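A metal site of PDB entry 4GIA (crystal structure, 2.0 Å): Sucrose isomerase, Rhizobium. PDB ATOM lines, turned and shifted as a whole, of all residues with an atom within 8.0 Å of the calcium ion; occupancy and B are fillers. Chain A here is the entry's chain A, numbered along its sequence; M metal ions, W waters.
Water W2 lies within hydrogen-bond range of the backbone carbonyl oxygen of Glu 75 and the side-chain amide nitrogen of Asn 24. Water W1 bridges the backbone carbonyl oxygen of Glu 75 (2.6 Å) and the side-chain carboxylate of Asp 26 (2.7 Å).
The side-chain carboxylate (OD1) of Asp 30 sits at hydrogen-bond distance from the side-chain hydroxyl (OG1) of Thr 23, 2.8 Å away. The side-chain carboxylate of Asp 22 sits at hydrogen-bond distance from the backbone NH of Gly 27 (2.9 Å). The side-chain carboxylate (OD2) of Asp 22 is in hydrogen-bond range of the backbone NH (N) of Gly 25 (3.4 Å). N of Gly 33 lies within hydrogen-bond range of OD1 of Asp 30. OD1 of Asp 30 lies close to N of Lys 32, 3.5 Å away. OD2 of Asp 22 lies within hydrogen-bond range of OG1 of Thr 432, at 2.6 Å. The backbone NH (N) of Asp 22 sits at hydrogen-bond distance from the backbone carbonyl oxygen (O) of Phe 431 (3.1 Å). The backbone carbonyl oxygen (O) of Lys 21 lies within hydrogen-bond range of the backbone NH (N) of Asp 30 (3.1 Å).
Of the 21 residues printed, 5 come within 4 Å of the calcium ion. Along chain A the residues within 4 Å of the calcium ion span positions 22 to 30. The nearest printed residue that does not touch the calcium ion is Thr 23 (4.2 Å).
The calcium ion is bound by water W1, the side-chain carboxylate of Asp 22, the backbone carbonyl oxygen of Ile 28, the side-chain carboxylate of Asp 30, the side-chain amide oxygen of Asn 24, the side-chain carboxylate of Asp 26 and water W2. The calcium ion has seven donor atoms within binding distance.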
ATOM      1  N   PRO A  17      23.925 -27.314  18.880  1.00  0.00           N
ATOM      2  CA  PRO A  17      24.555 -26.133  18.200  1.00  0.00           C
ATOM      3  C   PRO A  17      25.154 -25.137  19.164  1.00  0.00           C
ATOM      4  O   PRO A  17      26.149 -24.494  18.845  1.00  0.00           O
ATOM      5  CB  PRO A  17      23.382 -25.497  17.420  1.00  0.00           C
ATOM      6  CG  PRO A  17      22.371 -26.605  17.293  1.00  0.00           C
ATOM      7  CD  PRO A  17      22.490 -27.420  18.552  1.00  0.00           C
ATOM      8  N   ARG A  18      24.582 -25.050  20.363  1.00  0.00           N
ATOM      9  CA  ARG A  18      25.099 -24.136  21.403  1.00  0.00           C
ATOM     10  C   ARG A  18      26.602 -24.388  21.729  1.00  0.00           C
ATOM     11  O   ARG A  18      27.354 -23.483  22.136  1.00  0.00           O
ATOM     12  CB  ARG A  18      24.251 -24.396  22.648  1.00  0.00           C
ATOM     13  CG  ARG A  18      24.660 -23.648  23.883  1.00  0.00           C
ATOM     14  CD  ARG A  18      23.477 -23.533  24.833  1.00  0.00           C
ATOM     15  NE  ARG A  18      23.838 -22.623  25.896  1.00  0.00           N
ATOM     16  CZ  ARG A  18      23.406 -21.367  26.023  1.00  0.00           C
ATOM     17  NH1 ARG A  18      22.491 -20.859  25.204  1.00  0.00           N
ATOM     18  NH2 ARG A  18      23.873 -20.635  27.025  1.00  0.00           N
ATOM     19  N   LYS A  21      30.152 -24.798  17.328  1.00  0.00           N
ATOM     20  CA  LYS A  21      31.122 -23.808  16.818  1.00  0.00           C
ATOM     21  C   LYS A  21      30.563 -22.389  16.821  1.00  0.00           C
ATOM     22  O   LYS A  21      29.554 -22.134  16.168  1.00  0.00           O
ATOM     23  CB  LYS A  21      31.603 -24.195  15.413  1.00  0.00           C
ATOM     24  CG  LYS A  21      32.689 -23.288  14.793  1.00  0.00           C
ATOM     25  CD  LYS A  21      33.972 -23.298  15.631  1.00  0.00           C
ATOM     26  CE  LYS A  21      35.152 -22.515  15.017  1.00  0.00           C
ATOM     27  NZ  LYS A  21      34.724 -21.297  14.303  1.00  0.00           N
ATOM     28  N   ASP A  22      31.212 -21.491  17.572  1.00  0.00           N
ATOM     29  CA  ASP A  22      30.840 -20.068  17.673  1.00  0.00           C
ATOM     30  C   ASP A  22      31.632 -19.284  16.601  1.00  0.00           C
ATOM     31  O   ASP A  22      32.835 -19.487  16.468  1.00  0.00           O
ATOM     32  CB  ASP A  22      31.238 -19.534  19.053  1.00  0.00           C
ATOM     33  CG  ASP A  22      30.950 -18.042  19.240  1.00  0.00           C
ATOM     34  OD1 ASP A  22      30.159 -17.411  18.499  1.00  0.00           O
ATOM     35  OD2 ASP A  22      31.480 -17.485  20.235  1.00  0.00           O
ATOM     36  N   THR A  23      30.957 -18.395  15.879  1.00  0.00           N
ATOM     37  CA  THR A  23      31.631 -17.584  14.862  1.00  0.00           C
ATOM     38  C   THR A  23      31.525 -16.073  15.099  1.00  0.00           C
ATOM     39  O   THR A  23      31.848 -15.268  14.206  1.00  0.00           O
ATOM     40  CB  THR A  23      31.068 -17.857  13.465  1.00  0.00           C
ATOM     41  OG1 THR A  23      29.680 -17.484  13.458  1.00  0.00           O
ATOM     42  CG2 THR A  23      31.225 -19.322  13.085  1.00  0.00           C
ATOM     43  N   ASN A  24      31.066 -15.663  16.265  1.00  0.00           N
ATOM     44  CA  ASN A  24      30.964 -14.214  16.525  1.00  0.00           C
ATOM     45  C   ASN A  24      31.358 -13.753  17.934  1.00  0.00           C
ATOM     46  O   ASN A  24      30.916 -12.717  18.382  1.00  0.00           O
ATOM     47  CB  ASN A  24      29.571 -13.689  16.156  1.00  0.00           C
ATOM     48  CG  ASN A  24      28.517 -14.036  17.195  1.00  0.00           C
ATOM     49  OD1 ASN A  24      28.682 -14.978  17.983  1.00  0.00           O
ATOM     50  ND2 ASN A  24      27.443 -13.289  17.202  1.00  0.00           N
ATOM     51  N   GLY A  25      32.133 -14.554  18.645  1.00  0.00           N
ATOM     52  CA  GLY A  25      32.673 -14.183  19.929  1.00  0.00           C
ATOM     53  C   GLY A  25      31.764 -14.073  21.156  1.00  0.00           C
ATOM     54  O   GLY A  25      32.222 -13.627  22.202  1.00  0.00           O
ATOM     55  N   ASP A  26      30.491 -14.478  21.055  1.00  0.00           N
ATOM     56  CA  ASP A  26      29.628 -14.391  22.238  1.00  0.00           C
ATOM     57  C   ASP A  26      29.697 -15.632  23.153  1.00  0.00           C
ATOM     58  O   ASP A  26      28.999 -15.700  24.164  1.00  0.00           O
ATOM     59  CB  ASP A  26      28.187 -14.069  21.842  1.00  0.00           C
ATOM     60  CG  ASP A  26      27.505 -15.221  21.102  1.00  0.00           C
ATOM     61  OD1 ASP A  26      28.176 -16.217  20.728  1.00  0.00           O
ATOM     62  OD2 ASP A  26      26.271 -15.135  20.933  1.00  0.00           O
ATOM     63  N   GLY A  27      30.568 -16.577  22.824  1.00  0.00           N
ATOM     64  CA  GLY A  27      30.717 -17.793  23.623  1.00  0.00           C
ATOM     65  C   GLY A  27      29.675 -18.903  23.374  1.00  0.00           C
ATOM     66  O   GLY A  27      29.695 -19.946  24.050  1.00  0.00           O
ATOM     67  N   ILE A  28      28.785 -18.673  22.403  1.00  0.00           N
ATOM     68  CA  ILE A  28      27.676 -19.623  22.110  1.00  0.00           C
ATOM     69  C   ILE A  28      27.780 -20.073  20.646  1.00  0.00           C
ATOM     70  O   ILE A  28      27.910 -19.240  19.729  1.00  0.00           O
ATOM     71  CB  ILE A  28      26.288 -18.985  22.411  1.00  0.00           C
ATOM     72  CG1 ILE A  28      26.202 -18.596  23.898  1.00  0.00           C
ATOM     73  CG2 ILE A  28      25.111 -19.887  21.963  1.00  0.00           C
ATOM     74  CD1 ILE A  28      25.108 -17.608  24.245  1.00  0.00           C
ATOM     75  N   GLY A  29      27.694 -21.376  20.400  1.00  0.00           N
ATOM     76  CA  GLY A  29      27.735 -21.888  19.021  1.00  0.00           C
ATOM     77  C   GLY A  29      26.534 -21.441  18.195  1.00  0.00           C
ATOM     78  O   GLY A  29      25.511 -21.080  18.752  1.00  0.00           O
ATOM     79  N   ASP A  30      26.660 -21.458  16.869  1.00  0.00           N
ATOM     80  CA  ASP A  30      25.619 -20.856  16.019  1.00  0.00           C
ATOM     81  C   ASP A  30      25.530 -21.551  14.663  1.00  0.00           C
ATOM     82  O   ASP A  30      26.327 -22.454  14.365  1.00  0.00           O
ATOM     83  CB  ASP A  30      25.895 -19.334  15.871  1.00  0.00           C
ATOM     84  CG  ASP A  30      27.367 -19.028  15.535  1.00  0.00           C
ATOM     85  OD1 ASP A  30      27.830 -19.413  14.435  1.00  0.00           O
ATOM     86  OD2 ASP A  30      28.065 -18.353  16.346  1.00  0.00           O
ATOM     87  N   PHE A  31      24.579 -21.126  13.835  1.00  0.00           N
ATOM     88  CA  PHE A  31      24.330 -21.797  12.547  1.00  0.00           C
ATOM     89  C   PHE A  31      25.534 -21.610  11.625  1.00  0.00           C
ATOM     90  O   PHE A  31      25.950 -22.580  10.969  1.00  0.00           O
ATOM     91  CB  PHE A  31      23.069 -21.255  11.849  1.00  0.00           C
ATOM     92  CG  PHE A  31      21.762 -21.731  12.423  1.00  0.00           C
ATOM     93  CD1 PHE A  31      21.578 -23.056  12.819  1.00  0.00           C
ATOM     94  CD2 PHE A  31      20.689 -20.844  12.556  1.00  0.00           C
ATOM     95  CE1 PHE A  31      20.336 -23.489  13.292  1.00  0.00           C
ATOM     96  CE2 PHE A  31      19.460 -21.268  13.058  1.00  0.00           C
ATOM     97  CZ  PHE A  31      19.284 -22.600  13.418  1.00  0.00           C
ATOM     98  N   LYS A  32      26.111 -20.395  11.558  1.00  0.00           N
ATOM     99  CA  LYS A  32      27.269 -20.173  10.652  1.00  0.00           C
ATOM    100  C   LYS A  32      28.392 -21.111  11.034  1.00  0.00           C
ATOM    101  O   LYS A  32      29.064 -21.684  10.186  1.00  0.00           O
ATOM    102  CB  LYS A  32      27.842 -18.749  10.716  1.00  0.00           C
ATOM    103  CG  LYS A  32      26.869 -17.642  10.374  1.00  0.00           C
ATOM    104  N   GLY A  33      28.585 -21.281  12.346  1.00  0.00           N
ATOM    105  CA  GLY A  33      29.571 -22.249  12.842  1.00  0.00           C
ATOM    106  C   GLY A  33      29.325 -23.663  12.348  1.00  0.00           C
ATOM    107  O   GLY A  33      30.238 -24.332  11.889  1.00  0.00           O
ATOM    108  N   LYS A  74      17.560 -16.492  18.390  1.00  0.00           N
ATOM    109  CA  LYS A  74      18.379 -15.294  18.136  1.00  0.00           C
ATOM    110  C   LYS A  74      19.908 -15.581  18.204  1.00  0.00           C
ATOM    111  O   LYS A  74      20.642 -15.189  17.301  1.00  0.00           O
ATOM    112  CB  LYS A  74      17.976 -14.146  19.071  1.00  0.00           C
ATOM    113  N   GLU A  75      20.354 -16.293  19.240  1.00  0.00           N
ATOM    114  CA  GLU A  75      21.768 -16.715  19.371  1.00  0.00           C
ATOM    115  C   GLU A  75      22.293 -17.540  18.177  1.00  0.00           C
ATOM    116  O   GLU A  75      23.476 -17.469  17.876  1.00  0.00           O
ATOM    117  CB  GLU A  75      22.006 -17.513  20.657  1.00  0.00           C
ATOM    118  CG  GLU A  75      21.970 -16.721  21.940  1.00  0.00           C
ATOM    119  CD  GLU A  75      20.543 -16.433  22.422  1.00  0.00           C
ATOM    120  OE1 GLU A  75      19.553 -16.884  21.807  1.00  0.00           O
ATOM    121  OE2 GLU A  75      20.404 -15.758  23.458  1.00  0.00           O
ATOM    122  N   TYR A  76      21.434 -18.319  17.501  1.00  0.00           N
ATOM    123  CA  TYR A  76      21.922 -19.163  16.383  1.00  0.00           C
ATOM    124  C   TYR A  76      22.032 -18.433  15.016  1.00  0.00           C
ATOM    125  O   TYR A  76      22.853 -18.794  14.169  1.00  0.00           O
ATOM    126  CB  TYR A  76      21.110 -20.478  16.243  1.00  0.00           C
ATOM    127  CG  TYR A  76      21.173 -21.384  17.471  1.00  0.00           C
ATOM    128  CD1 TYR A  76      22.106 -21.143  18.492  1.00  0.00           C
ATOM    129  CD2 TYR A  76      20.308 -22.486  17.619  1.00  0.00           C
ATOM    130  CE1 TYR A  76      22.158 -21.951  19.623  1.00  0.00           C
ATOM    131  CE2 TYR A  76      20.361 -23.304  18.748  1.00  0.00           C
ATOM    132  CZ  TYR A  76      21.284 -23.012  19.752  1.00  0.00           C
ATOM    133  OH  TYR A  76      21.398 -23.797  20.894  1.00  0.00           O
ATOM    134  N   GLY A  77      21.196 -17.420  14.819  1.00  0.00           N
ATOM    135  CA  GLY A  77      21.291 -16.566  13.633  1.00  0.00           C
ATOM    136  C   GLY A  77      19.894 -16.148  13.211  1.00  0.00           C
ATOM    137  O   GLY A  77      19.029 -15.883  14.083  1.00  0.00           O
ATOM    138  N   PHE A 431      36.896 -23.266  19.815  1.00  0.00           N
ATOM    139  CA  PHE A 431      35.416 -23.179  19.781  1.00  0.00           C
ATOM    140  C   PHE A 431      34.974 -21.726  19.591  1.00  0.00           C
ATOM    141  O   PHE A 431      34.074 -21.439  18.781  1.00  0.00           O
ATOM    142  CB  PHE A 431      34.820 -23.825  21.056  1.00  0.00           C
ATOM    143  CG  PHE A 431      33.404 -23.401  21.365  1.00  0.00           C
ATOM    144  CD1 PHE A 431      32.334 -23.833  20.579  1.00  0.00           C
ATOM    145  CD2 PHE A 431      33.131 -22.568  22.446  1.00  0.00           C
ATOM    146  CE1 PHE A 431      31.034 -23.439  20.861  1.00  0.00           C
ATOM    147  CE2 PHE A 431      31.819 -22.196  22.740  1.00  0.00           C
ATOM    148  CZ  PHE A 431      30.762 -22.616  21.941  1.00  0.00           C
ATOM    149  N   THR A 432      35.651 -20.802  20.303  1.00  0.00           N
ATOM    150  CA  THR A 432      35.274 -19.385  20.353  1.00  0.00           C
ATOM    151  C   THR A 432      36.488 -18.442  20.479  1.00  0.00           C
ATOM    152  O   THR A 432      37.532 -18.837  21.028  1.00  0.00           O
ATOM    153  CB  THR A 432      34.286 -19.125  21.534  1.00  0.00           C
ATOM    154  OG1 THR A 432      33.771 -17.797  21.452  1.00  0.00           O
ATOM    155  CG2 THR A 432      34.933 -19.316  22.885  1.00  0.00           C
HETATM  156 CA    CA M   1      27.820 -17.217  18.492  1.00  0.00          CA
HETATM  157  O   HOH W   1      25.743 -17.063  19.156  1.00  0.00           O
HETATM  158  O   HOH W   2      26.073 -16.075  17.080  1.00  0.00           O
